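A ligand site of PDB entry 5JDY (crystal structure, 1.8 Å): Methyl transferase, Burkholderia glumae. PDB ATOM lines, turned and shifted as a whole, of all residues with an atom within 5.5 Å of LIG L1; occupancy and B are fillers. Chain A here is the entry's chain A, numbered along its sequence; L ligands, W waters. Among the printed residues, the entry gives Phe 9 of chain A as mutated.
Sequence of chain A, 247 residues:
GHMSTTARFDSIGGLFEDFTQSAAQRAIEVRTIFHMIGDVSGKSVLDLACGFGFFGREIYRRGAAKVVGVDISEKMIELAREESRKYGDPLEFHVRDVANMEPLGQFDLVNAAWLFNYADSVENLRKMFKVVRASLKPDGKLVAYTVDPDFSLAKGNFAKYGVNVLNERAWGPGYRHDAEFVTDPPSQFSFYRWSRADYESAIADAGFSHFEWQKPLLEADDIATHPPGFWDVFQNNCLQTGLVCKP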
ATOM      1  N   ALA A   7     -20.456   1.071 -19.997  1.00  0.00           N
ATOM      2  CA  ALA A   7     -19.091   0.906 -19.507  1.00  0.00           C
ATOM      3  C   ALA A   7     -19.025  -0.191 -18.456  1.00  0.00           C
ATOM      4  O   ALA A   7     -19.828  -0.180 -17.514  1.00  0.00           O
ATOM      5  CB  ALA A   7     -18.563   2.231 -18.934  1.00  0.00           C
ATOM      6  N   PHE A   9     -17.028  -0.776 -16.013  1.00  0.00           N
ATOM      7  CA  PHE A   9     -16.765  -0.391 -14.636  1.00  0.00           C
ATOM      8  C   PHE A   9     -17.939   0.325 -13.984  1.00  0.00           C
ATOM      9  O   PHE A   9     -17.883   0.589 -12.781  1.00  0.00           O
ATOM     10  CB  PHE A   9     -15.489   0.445 -14.556  1.00  0.00           C
ATOM     11  CG  PHE A   9     -14.232  -0.371 -14.475  1.00  0.00           C
ATOM     12  CD1 PHE A   9     -13.492  -0.431 -13.308  1.00  0.00           C
ATOM     13  CD2 PHE A   9     -13.818  -1.125 -15.570  1.00  0.00           C
ATOM     14  CE1 PHE A   9     -12.314  -1.194 -13.231  1.00  0.00           C
ATOM     15  CE2 PHE A   9     -12.668  -1.898 -15.495  1.00  0.00           C
ATOM     16  CZ  PHE A   9     -11.908  -1.930 -14.314  1.00  0.00           C
ATOM     17  N   PHE A  16     -13.340  -1.560  -7.211  1.00  0.00           N
ATOM     18  CA  PHE A  16     -11.978  -1.446  -7.722  1.00  0.00           C
ATOM     19  C   PHE A  16     -11.027  -0.896  -6.662  1.00  0.00           C
ATOM     20  O   PHE A  16      -9.914  -1.411  -6.496  1.00  0.00           O
ATOM     21  CB  PHE A  16     -11.928  -0.570  -8.986  1.00  0.00           C
ATOM     22  CG  PHE A  16     -10.529  -0.447  -9.522  1.00  0.00           C
ATOM     23  CD1 PHE A  16      -9.891  -1.548 -10.103  1.00  0.00           C
ATOM     24  CD2 PHE A  16      -9.836   0.729  -9.399  1.00  0.00           C
ATOM     25  CE1 PHE A  16      -8.584  -1.460 -10.571  1.00  0.00           C
ATOM     26  CE2 PHE A  16      -8.523   0.829  -9.867  1.00  0.00           C
ATOM     27  CZ  PHE A  16      -7.902  -0.270 -10.462  1.00  0.00           C
ATOM     28  N   THR A  20      -7.596  -2.426  -4.978  1.00  0.00           N
ATOM     29  CA  THR A  20      -6.279  -1.808  -4.860  1.00  0.00           C
ATOM     30  C   THR A  20      -5.736  -1.889  -3.439  1.00  0.00           C
ATOM     31  O   THR A  20      -4.504  -1.857  -3.260  1.00  0.00           O
ATOM     32  CB  THR A  20      -6.265  -0.340  -5.317  1.00  0.00           C
ATOM     33  OG1 THR A  20      -6.994   0.477  -4.395  1.00  0.00           O
ATOM     34  CG2 THR A  20      -6.829  -0.166  -6.715  1.00  0.00           C
ATOM     35  N   ARG A  26      -0.628  -4.691  -6.344  1.00  0.00           N
ATOM     36  CA  ARG A  26      -0.867  -3.260  -6.514  1.00  0.00           C
ATOM     37  C   ARG A  26       0.342  -2.423  -6.058  1.00  0.00           C
ATOM     38  O   ARG A  26       0.724  -1.457  -6.731  1.00  0.00           O
ATOM     39  CB  ARG A  26      -2.135  -2.822  -5.773  1.00  0.00           C
ATOM     40  CG  ARG A  26      -2.467  -1.332  -5.936  1.00  0.00           C
ATOM     41  CD  ARG A  26      -2.660  -0.861  -7.406  1.00  0.00           C
ATOM     42  NE  ARG A  26      -3.258   0.479  -7.422  1.00  0.00           N
ATOM     43  CZ  ARG A  26      -3.814   1.060  -8.474  1.00  0.00           C
ATOM     44  NH1 ARG A  26      -3.853   0.449  -9.655  1.00  0.00           N
ATOM     45  NH2 ARG A  26      -4.338   2.271  -8.334  1.00  0.00           N
ATOM     46  N   GLU A  29       2.794  -2.338  -8.930  1.00  0.00           N
ATOM     47  CA  GLU A  29       2.323  -1.414  -9.966  1.00  0.00           C
ATOM     48  C   GLU A  29       2.611   0.028  -9.596  1.00  0.00           C
ATOM     49  O   GLU A  29       3.176   0.795 -10.384  1.00  0.00           O
ATOM     50  CB  GLU A  29       0.798  -1.533 -10.179  1.00  0.00           C
ATOM     51  CG  GLU A  29       0.220  -2.861 -10.634  1.00  0.00           C
ATOM     52  CD  GLU A  29      -1.304  -2.927 -10.458  1.00  0.00           C
ATOM     53  OE1 GLU A  29      -2.017  -1.886 -10.625  1.00  0.00           O
ATOM     54  OE2 GLU A  29      -1.787  -4.020 -10.138  1.00  0.00           O
ATOM     55  N   ASP A  47      -4.320  12.122 -17.017  1.00  0.00           N
ATOM     56  CA  ASP A  47      -4.396  10.786 -16.418  1.00  0.00           C
ATOM     57  C   ASP A  47      -5.548  10.057 -17.117  1.00  0.00           C
ATOM     58  O   ASP A  47      -6.722  10.377 -16.876  1.00  0.00           O
ATOM     59  CB  ASP A  47      -4.627  10.894 -14.910  1.00  0.00           C
ATOM     60  CG  ASP A  47      -4.559   9.550 -14.204  1.00  0.00           C
ATOM     61  OD1 ASP A  47      -3.843   8.644 -14.672  1.00  0.00           O
ATOM     62  OD2 ASP A  47      -5.205   9.397 -13.148  1.00  0.00           O
ATOM     63  N   LEU A  48      -5.208   9.126 -17.985  1.00  0.00           N
ATOM     64  CA  LEU A  48      -6.177   8.452 -18.832  1.00  0.00           C
ATOM     65  C   LEU A  48      -6.547   7.104 -18.227  1.00  0.00           C
ATOM     66  O   LEU A  48      -5.707   6.441 -17.601  1.00  0.00           O
ATOM     67  CB  LEU A  48      -5.642   8.239 -20.252  1.00  0.00           C
ATOM     68  CG  LEU A  48      -5.292   9.508 -21.055  1.00  0.00           C
ATOM     69  CD1 LEU A  48      -4.665   9.109 -22.375  1.00  0.00           C
ATOM     70  CD2 LEU A  48      -6.530  10.395 -21.299  1.00  0.00           C
ATOM     71  N   ALA A  49      -7.794   6.706 -18.448  1.00  0.00           N
ATOM     72  CA  ALA A  49      -8.396   5.566 -17.746  1.00  0.00           C
ATOM     73  C   ALA A  49      -8.202   5.758 -16.238  1.00  0.00           C
ATOM     74  O   ALA A  49      -7.710   4.873 -15.529  1.00  0.00           O
ATOM     75  CB  ALA A  49      -7.810   4.238 -18.247  1.00  0.00           C
ATOM     76  N   CYS A  50      -8.585   6.930 -15.757  1.00  0.00           N
ATOM     77  CA  CYS A  50      -8.177   7.360 -14.420  1.00  0.00           C
ATOM     78  C   CYS A  50      -8.893   6.637 -13.290  1.00  0.00           C
ATOM     79  O   CYS A  50      -8.437   6.728 -12.147  1.00  0.00           O
ATOM     80  CB  CYS A  50      -8.391   8.877 -14.247  1.00  0.00           C
ATOM     81  SG  CYS A  50     -10.092   9.416 -14.404  1.00  0.00           S
ATOM     82  N   GLY A  51      -9.979   5.903 -13.565  1.00  0.00           N
ATOM     83  CA  GLY A  51     -10.721   5.252 -12.487  1.00  0.00           C
ATOM     84  C   GLY A  51     -11.213   6.272 -11.484  1.00  0.00           C
ATOM     85  O   GLY A  51     -11.742   7.327 -11.857  1.00  0.00           O
ATOM     86  N   PHE A  52     -11.043   5.971 -10.186  1.00  0.00           N
ATOM     87  CA  PHE A  52     -11.414   6.983  -9.198  1.00  0.00           C
ATOM     88  C   PHE A  52     -10.358   8.066  -9.057  1.00  0.00           C
ATOM     89  O   PHE A  52     -10.514   8.945  -8.208  1.00  0.00           O
ATOM     90  CB  PHE A  52     -11.722   6.358  -7.834  1.00  0.00           C
ATOM     91  CG  PHE A  52     -10.580   5.558  -7.239  1.00  0.00           C
ATOM     92  CD1 PHE A  52      -9.650   6.165  -6.410  1.00  0.00           C
ATOM     93  CD2 PHE A  52     -10.455   4.183  -7.484  1.00  0.00           C
ATOM     94  CE1 PHE A  52      -8.620   5.452  -5.846  1.00  0.00           C
ATOM     95  CE2 PHE A  52      -9.414   3.442  -6.922  1.00  0.00           C
ATOM     96  CZ  PHE A  52      -8.474   4.099  -6.085  1.00  0.00           C
ATOM     97  N   PHE A  54      -6.749   7.682  -8.790  1.00  0.00           N
ATOM     98  CA  PHE A  54      -5.641   7.428  -7.867  1.00  0.00           C
ATOM     99  C   PHE A  54      -4.351   8.096  -8.329  1.00  0.00           C
ATOM    100  O   PHE A  54      -3.721   8.851  -7.574  1.00  0.00           O
ATOM    101  CB  PHE A  54      -5.379   5.930  -7.691  1.00  0.00           C
ATOM    102  CG  PHE A  54      -4.199   5.660  -6.785  1.00  0.00           C
ATOM    103  CD1 PHE A  54      -4.341   5.717  -5.414  1.00  0.00           C
ATOM    104  CD2 PHE A  54      -2.929   5.452  -7.331  1.00  0.00           C
ATOM    105  CE1 PHE A  54      -3.258   5.524  -4.587  1.00  0.00           C
ATOM    106  CE2 PHE A  54      -1.841   5.258  -6.517  1.00  0.00           C
ATOM    107  CZ  PHE A  54      -1.994   5.296  -5.141  1.00  0.00           C
ATOM    108  N   PHE A  55      -3.928   7.831  -9.567  1.00  0.00           N
ATOM    109  CA  PHE A  55      -2.611   8.285  -9.981  1.00  0.00           C
ATOM    110  C   PHE A  55      -2.574   9.793 -10.176  1.00  0.00           C
ATOM    111  O   PHE A  55      -1.657  10.458  -9.688  1.00  0.00           O
ATOM    112  CB  PHE A  55      -2.154   7.542 -11.227  1.00  0.00           C
ATOM    113  CG  PHE A  55      -1.722   6.147 -10.928  1.00  0.00           C
ATOM    114  CD1 PHE A  55      -0.510   5.928 -10.278  1.00  0.00           C
ATOM    115  CD2 PHE A  55      -2.559   5.079 -11.208  1.00  0.00           C
ATOM    116  CE1 PHE A  55      -0.106   4.639  -9.951  1.00  0.00           C
ATOM    117  CE2 PHE A  55      -2.170   3.781 -10.886  1.00  0.00           C
ATOM    118  CZ  PHE A  55      -0.948   3.566 -10.256  1.00  0.00           C
ATOM    119  N   VAL A  70      -9.455  11.372 -17.300  1.00  0.00           N
ATOM    120  CA  VAL A  70     -10.431  10.930 -18.309  1.00  0.00           C
ATOM    121  C   VAL A  70     -10.735   9.457 -18.086  1.00  0.00           C
ATOM    122  O   VAL A  70      -9.823   8.644 -17.914  1.00  0.00           O
ATOM    123  CB  VAL A  70      -9.908  11.134 -19.761  1.00  0.00           C
ATOM    124  CG1 VAL A  70     -10.965  10.699 -20.770  1.00  0.00           C
ATOM    125  CG2 VAL A  70      -9.481  12.582 -19.997  1.00  0.00           C
ATOM    126  N   ASP A  71     -12.024   9.099 -18.121  1.00  0.00           N
ATOM    127  CA  ASP A  71     -12.455   7.710 -17.981  1.00  0.00           C
ATOM    128  C   ASP A  71     -13.731   7.504 -18.776  1.00  0.00           C
ATOM    129  O   ASP A  71     -14.572   8.401 -18.868  1.00  0.00           O
ATOM    130  CB  ASP A  71     -12.693   7.324 -16.517  1.00  0.00           C
ATOM    131  CG  ASP A  71     -12.620   5.840 -16.299  1.00  0.00           C
ATOM    132  OD1 ASP A  71     -11.539   5.374 -15.930  1.00  0.00           O
ATOM    133  OD2 ASP A  71     -13.630   5.115 -16.545  1.00  0.00           O
ATOM    134  N   ILE A  72     -13.883   6.310 -19.348  1.00  0.00           N
ATOM    135  CA  ILE A  72     -15.086   6.004 -20.124  1.00  0.00           C
ATOM    136  C   ILE A  72     -16.308   5.809 -19.232  1.00  0.00           C
ATOM    137  O   ILE A  72     -17.448   5.937 -19.705  1.00  0.00           O
ATOM    138  CB  ILE A  72     -14.844   4.775 -21.008  1.00  0.00           C
ATOM    139  CG1 ILE A  72     -15.866   4.705 -22.142  1.00  0.00           C
ATOM    140  CG2 ILE A  72     -14.848   3.480 -20.151  1.00  0.00           C
ATOM    141  CD1 ILE A  72     -15.584   3.620 -23.150  1.00  0.00           C
ATOM    142  N   SER A  73     -16.111   5.582 -17.936  1.00  0.00           N
ATOM    143  CA  SER A  73     -17.183   5.174 -17.034  1.00  0.00           C
ATOM    144  C   SER A  73     -17.758   6.369 -16.285  1.00  0.00           C
ATOM    145  O   SER A  73     -17.065   6.988 -15.476  1.00  0.00           O
ATOM    146  CB  SER A  73     -16.661   4.136 -16.031  1.00  0.00           C
ATOM    147  OG  SER A  73     -17.631   3.910 -15.006  1.00  0.00           O
ATOM    148  N   MET A  76     -17.398   5.720 -12.492  1.00  0.00           N
ATOM    149  CA  MET A  76     -16.048   5.904 -11.970  1.00  0.00           C
ATOM    150  C   MET A  76     -15.700   7.386 -11.875  1.00  0.00           C
ATOM    151  O   MET A  76     -15.031   7.806 -10.932  1.00  0.00           O
ATOM    152  CB  MET A  76     -15.023   5.189 -12.873  1.00  0.00           C
ATOM    153  CG  MET A  76     -15.065   3.656 -12.874  1.00  0.00           C
ATOM    154  SD  MET A  76     -15.104   2.830 -11.247  1.00  0.00           S
ATOM    155  CE  MET A  76     -13.401   3.016 -10.739  1.00  0.00           C
ATOM    156  N   ARG A  96     -15.023  10.154 -21.244  1.00  0.00           N
ATOM    157  CA  ARG A  96     -14.746   9.969 -22.670  1.00  0.00           C
ATOM    158  C   ARG A  96     -14.243   8.557 -22.894  1.00  0.00           C
ATOM    159  O   ARG A  96     -13.552   7.988 -22.043  1.00  0.00           O
ATOM    160  CB  ARG A  96     -13.656  10.896 -23.223  1.00  0.00           C
ATOM    161  CG  ARG A  96     -13.829  12.385 -23.041  1.00  0.00           C
ATOM    162  CD  ARG A  96     -14.697  13.034 -24.092  1.00  0.00           C
ATOM    163  NE  ARG A  96     -14.569  14.486 -23.992  1.00  0.00           N
ATOM    164  CZ  ARG A  96     -15.230  15.227 -23.101  1.00  0.00           C
ATOM    165  NH1 ARG A  96     -16.067  14.653 -22.252  1.00  0.00           N
ATOM    166  NH2 ARG A  96     -15.048  16.543 -23.071  1.00  0.00           N
ATOM    167  N   ASP A  97     -14.506   8.028 -24.095  1.00  0.00           N
ATOM    168  CA  ASP A  97     -13.773   6.868 -24.600  1.00  0.00           C
ATOM    169  C   ASP A  97     -12.510   7.365 -25.271  1.00  0.00           C
ATOM    170  O   ASP A  97     -12.566   8.063 -26.291  1.00  0.00           O
ATOM    171  CB  ASP A  97     -14.660   6.057 -25.558  1.00  0.00           C
ATOM    172  CG  ASP A  97     -13.891   4.969 -26.326  1.00  0.00           C
ATOM    173  OD1 ASP A  97     -12.688   4.734 -26.086  1.00  0.00           O
ATOM    174  OD2 ASP A  97     -14.521   4.335 -27.194  1.00  0.00           O
ATOM    175  N   VAL A  98     -11.353   6.986 -24.714  1.00  0.00           N
ATOM    176  CA  VAL A  98     -10.082   7.549 -25.145  1.00  0.00           C
ATOM    177  C   VAL A  98      -9.789   7.187 -26.598  1.00  0.00           C
ATOM    178  O   VAL A  98      -9.115   7.942 -27.315  1.00  0.00           O
ATOM    179  CB  VAL A  98      -8.953   7.095 -24.200  1.00  0.00           C
ATOM    180  CG1 VAL A  98      -7.601   7.332 -24.799  1.00  0.00           C
ATOM    181  CG2 VAL A  98      -9.063   7.829 -22.849  1.00  0.00           C
ATOM    182  N   ALA A  99     -10.335   6.075 -27.093  1.00  0.00           N
ATOM    183  CA  ALA A  99     -10.095   5.700 -28.490  1.00  0.00           C
ATOM    184  C   ALA A  99     -10.729   6.672 -29.476  1.00  0.00           C
ATOM    185  O   ALA A  99     -10.266   6.770 -30.619  1.00  0.00           O
ATOM    186  CB  ALA A  99     -10.633   4.303 -28.774  1.00  0.00           C
ATOM    187  N   ALA A 113      -2.395   4.282 -16.801  1.00  0.00           N
ATOM    188  CA  ALA A 113      -2.289   3.053 -16.014  1.00  0.00           C
ATOM    189  C   ALA A 113      -3.523   2.216 -16.291  1.00  0.00           C
ATOM    190  O   ALA A 113      -4.611   2.535 -15.822  1.00  0.00           O
ATOM    191  CB  ALA A 113      -2.131   3.389 -14.530  1.00  0.00           C
ATOM    192  N   TRP A 114      -3.347   1.142 -17.081  1.00  0.00           N
ATOM    193  CA  TRP A 114      -4.436   0.213 -17.419  1.00  0.00           C
ATOM    194  C   TRP A 114      -5.439   0.853 -18.383  1.00  0.00           C
ATOM    195  O   TRP A 114      -6.656   0.791 -18.192  1.00  0.00           O
ATOM    196  CB  TRP A 114      -5.114  -0.338 -16.166  1.00  0.00           C
ATOM    197  CG  TRP A 114      -4.165  -1.020 -15.242  1.00  0.00           C
ATOM    198  CD1 TRP A 114      -3.811  -0.618 -13.984  1.00  0.00           C
ATOM    199  CD2 TRP A 114      -3.438  -2.227 -15.496  1.00  0.00           C
ATOM    200  NE1 TRP A 114      -2.908  -1.505 -13.440  1.00  0.00           N
ATOM    201  CE2 TRP A 114      -2.661  -2.507 -14.345  1.00  0.00           C
ATOM    202  CE3 TRP A 114      -3.369  -3.118 -16.588  1.00  0.00           C
ATOM    203  CZ2 TRP A 114      -1.839  -3.640 -14.237  1.00  0.00           C
ATOM    204  CZ3 TRP A 114      -2.550  -4.241 -16.489  1.00  0.00           C
ATOM    205  CH2 TRP A 114      -1.802  -4.493 -15.321  1.00  0.00           C
ATOM    206  N   LEU A 115      -4.908   1.482 -19.438  1.00  0.00           N
ATOM    207  CA  LEU A 115      -5.722   1.956 -20.547  1.00  0.00           C
ATOM    208  C   LEU A 115      -5.663   1.026 -21.753  1.00  0.00           C
ATOM    209  O   LEU A 115      -6.699   0.541 -22.223  1.00  0.00           O
ATOM    210  CB  LEU A 115      -5.279   3.367 -20.956  1.00  0.00           C
ATOM    211  CG  LEU A 115      -5.875   3.818 -22.309  1.00  0.00           C
ATOM    212  CD1 LEU A 115      -7.379   4.068 -22.169  1.00  0.00           C
ATOM    213  CD2 LEU A 115      -5.130   5.039 -22.850  1.00  0.00           C
ATOM    214  N   TYR A 118      -7.560  -2.222 -22.547  1.00  0.00           N
ATOM    215  CA  TYR A 118      -8.994  -2.147 -22.771  1.00  0.00           C
ATOM    216  C   TYR A 118      -9.341  -1.774 -24.192  1.00  0.00           C
ATOM    217  O   TYR A 118     -10.526  -1.725 -24.533  1.00  0.00           O
ATOM    218  CB  TYR A 118      -9.632  -1.177 -21.765  1.00  0.00           C
ATOM    219  CG  TYR A 118      -9.584  -1.760 -20.372  1.00  0.00           C
ATOM    220  CD1 TYR A 118     -10.295  -2.917 -20.071  1.00  0.00           C
ATOM    221  CD2 TYR A 118      -8.805  -1.194 -19.368  1.00  0.00           C
ATOM    222  CE1 TYR A 118     -10.229  -3.502 -18.814  1.00  0.00           C
ATOM    223  CE2 TYR A 118      -8.738  -1.765 -18.097  1.00  0.00           C
ATOM    224  CZ  TYR A 118      -9.465  -2.911 -17.833  1.00  0.00           C
ATOM    225  OH  TYR A 118      -9.401  -3.480 -16.578  1.00  0.00           O
ATOM    226  N   MET A 128      -5.834   4.823 -29.965  1.00  0.00           N
ATOM    227  CA  MET A 128      -5.493   5.325 -28.635  1.00  0.00           C
ATOM    228  C   MET A 128      -4.092   5.938 -28.614  1.00  0.00           C
ATOM    229  O   MET A 128      -3.886   7.012 -28.031  1.00  0.00           O
ATOM    230  CB  MET A 128      -5.599   4.208 -27.594  1.00  0.00           C
ATOM    231  CG  MET A 128      -7.004   3.800 -27.230  1.00  0.00           C
ATOM    232  SD  MET A 128      -6.952   2.687 -25.806  1.00  0.00           S
ATOM    233  CE  MET A 128      -8.711   2.325 -25.568  1.00  0.00           C
HETATM  234  N1  LIG L   1      -5.893   3.922 -13.813  1.00  0.00           N
HETATM  235  C1  LIG L   1      -6.726   3.722 -12.589  1.00  0.00           C
HETATM  236  C2  LIG L   1      -7.959   2.855 -12.878  1.00  0.00           C
HETATM  237  C3  LIG L   1      -7.622   1.536 -13.547  1.00  0.00           C
HETATM  238  S1  LIG L   1      -9.149   0.642 -13.761  1.00  0.00           S
HETATM  239  C4  LIG L   1      -5.853   3.079 -11.544  1.00  0.00           C
HETATM  240  O1  LIG L   1      -6.001   3.298 -10.338  1.00  0.00           O
HETATM  241  O2  LIG L   1      -4.935   2.317 -11.887  1.00  0.00           O
HETATM  242  C5  LIG L   1      -9.389   0.709 -15.508  1.00  0.00           C
HETATM  243  C6  LIG L   1     -10.197   1.951 -15.897  1.00  0.00           C
HETATM  244  O3  LIG L   1     -10.108   2.120 -17.326  1.00  0.00           O
HETATM  245  C7  LIG L   1     -11.694   1.856 -15.558  1.00  0.00           C
HETATM  246  O4  LIG L   1     -12.062   2.987 -14.751  1.00  0.00           O
HETATM  247  C8  LIG L   1     -12.373   1.876 -16.927  1.00  0.00           C
HETATM  248  O5  LIG L   1     -13.692   2.443 -16.960  1.00  0.00           O
HETATM  249  C9  LIG L   1     -11.374   2.640 -17.759  1.00  0.00           C
HETATM  250  N2  LIG L   1     -11.496   2.458 -19.226  1.00  0.00           N
HETATM  251  C10 LIG L   1     -11.665   1.288 -19.873  1.00  0.00           C
HETATM  252  N3  LIG L   1     -11.732   1.498 -21.218  1.00  0.00           N
HETATM  253  C11 LIG L   1     -11.604   2.817 -21.434  1.00  0.00           C
HETATM  254  C12 LIG L   1     -11.584   3.693 -22.627  1.00  0.00           C
HETATM  255  N4  LIG L   1     -11.715   3.161 -23.862  1.00  0.00           N
HETATM  256  N5  LIG L   1     -11.430   5.012 -22.433  1.00  0.00           N
HETATM  257  C13 LIG L   1     -11.296   5.533 -21.189  1.00  0.00           C
HETATM  258  N6  LIG L   1     -11.310   4.803 -20.065  1.00  0.00           N
HETATM  259  C14 LIG L   1     -11.450   3.448 -20.130  1.00  0.00           C
HETATM  260  C1  LG2 L   2      -4.762  -6.293 -14.483  1.00  0.00           C
HETATM  261  O1  LG2 L   2      -3.963  -7.114 -14.103  1.00  0.00           O
HETATM  262  C2  LG2 L   2      -5.119  -5.109 -13.698  1.00  0.00           C
HETATM  263  O2  LG2 L   2      -6.797  -5.686 -17.191  1.00  0.00           O
HETATM  264  N1  LG2 L   2      -4.597  -4.834 -12.513  1.00  0.00           N
HETATM  265  C3  LG2 L   2      -4.953  -3.729 -11.889  1.00  0.00           C
HETATM  266  N2  LG2 L   2      -5.832  -2.890 -12.375  1.00  0.00           N
HETATM  267  N3  LG2 L   2      -6.386  -3.091 -13.532  1.00  0.00           N
HETATM  268  C4  LG2 L   2      -6.055  -4.198 -14.248  1.00  0.00           C
HETATM  269  N4  LG2 L   2      -6.614  -4.442 -15.419  1.00  0.00           N
HETATM  270  C5  LG2 L   2      -6.266  -5.521 -16.108  1.00  0.00           C
HETATM  271  N5  LG2 L   2      -5.375  -6.430 -15.681  1.00  0.00           N
HETATM  272  C6  LG2 L   2      -7.366  -2.167 -14.076  1.00  0.00           C
HETATM  273  C7  LG2 L   2      -5.079  -7.603 -16.511  1.00  0.00           C
HETATM  274  O   HOH W   1     -15.619   0.733 -18.013  1.00  0.00           O
HETATM  275  O   HOH W   2      -4.347   5.949 -15.293  1.00  0.00           O
HETATM  276  O   HOH W   3      -5.569   6.917 -11.950  1.00  0.00           O
HETATM  277  O   HOH W   4     -13.566  -0.492 -21.878  1.00  0.00           O
HETATM  278  O   HOH W   5      -8.132   4.973  -9.469  1.00  0.00           O
HETATM  279  O   HOH W   6     -13.634  -1.419 -19.152  1.00  0.00           O
HETATM  280  O   HOH W   7     -12.287   0.435 -24.709  1.00  0.00           O
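A nitrogen (N1) of LIG L1 is in hydrogen-bond range of the backbone carbonyl oxygen of Ala 49 (2.7 Å). N of Val 98 sits at hydrogen-bond distance from N5 of LIG L1 (3.0 Å). The backbone carbonyl oxygen (O) of Ala 113 lies within hydrogen-bond range of a nitrogen (N1) of LIG L1 (2.8 Å). N6 of LIG L1 sits at hydrogen-bond distance from N of Ile 72 (3.1 Å). O5 of LIG L1 lies within hydrogen-bond range of OD2 of Asp 71 (2.7 Å). OD1 of Asp 97 sits at hydrogen-bond distance from N4 of LIG L1, 2.9 Å away. NE1 of Trp 114 lies close to N2 of LG2 L2, at 3.4 Å. O1 of LIG L1 lies within salt-bridge range of NH2 of Arg 26, at 2.8 Å. The side-chain hydroxyl of Tyr 118 is in hydrogen-bond range of a nitrogen (N4) of LG2 L2 (3.2 Å).
O of Asp 71 lies within hydrogen-bond range of N of Arg 96. N of Ile 72 lies close to O of Arg 96 (3.2 Å). The side-chain carboxylate of Glu 29 is in hydrogen-bond range of the indole nitrogen of Trp 114. N of Ala 49 is in hydrogen-bond range of O of Val 70. OG of Ser 73 lies within hydrogen-bond range of N of Met 76 (3.1 Å). N of Ser 73 lies within hydrogen-bond range of OD2 of Asp 71 (2.9 Å). The backbone NH (N) of Ala 99 is in hydrogen-bond range of the side-chain carboxylate (OD1) of Asp 97 (2.9 Å). The backbone NH (N) of Gly 51 is in hydrogen-bond range of the side-chain carboxylate (OD1) of Asp 71 (2.9 Å).
Phe 9 touches LIG L1. CE2 of Phe 16 touches O1 of LIG L1 (3.6 Å). O of Cys 50 touches C1 of LIG L1, at 3.5 Å. CA of Gly 51 touches O4 of LIG L1 (3.5 Å). Phe 54 touches LIG L1. CE2 of Phe 55 touches O2 of LIG L1, at 3.3 Å. CB of Ser 73 touches O5 of LIG L1, 3.5 Å away. CG of Met 76 touches O4 of LIG L1, 3.6 Å away. Arg 96 touches LIG L1 (O to C13, 3.4 Å). Trp 114 touches LIG L1. Tyr 118 touches LIG L1. CE of Met 128 touches N4 of LIG L1 (3.6 Å). Of the 28 residues printed, 19 come within 4 Å of LIG L1.
Water W1 bridges O5 of LIG L1 and N of Phe 9. Water W5 lies within hydrogen-bond range of an oxygen (O1) of LIG L1 (2.8 Å), the backbone NH (N) of Phe 54 (3.1 Å), the backbone NH (N) of Phe 52 (3.2 Å) and the backbone carbonyl oxygen (O) of Cys 50 (3.2 Å). Water W7 lies within hydrogen-bond range of the backbone carbonyl oxygen of Tyr 118 (2.8 Å) and a nitrogen (N4) of LIG L1 (2.9 Å). Water W2 lies within hydrogen-bond range of the backbone carbonyl oxygen of Leu 48 (2.7 Å), the side-chain carboxylate of Asp 47 (2.8 Å), a nitrogen (N1) of LIG L1 (2.9 Å) and the backbone NH of Ala 113 (3.0 Å). Water W3 lies within hydrogen-bond range of the side-chain carboxylate (OD2) of Asp 47, the backbone carbonyl oxygen (O) of Cys 50, the backbone NH (N) of Phe 55 and the backbone NH (N) of Phe 54.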
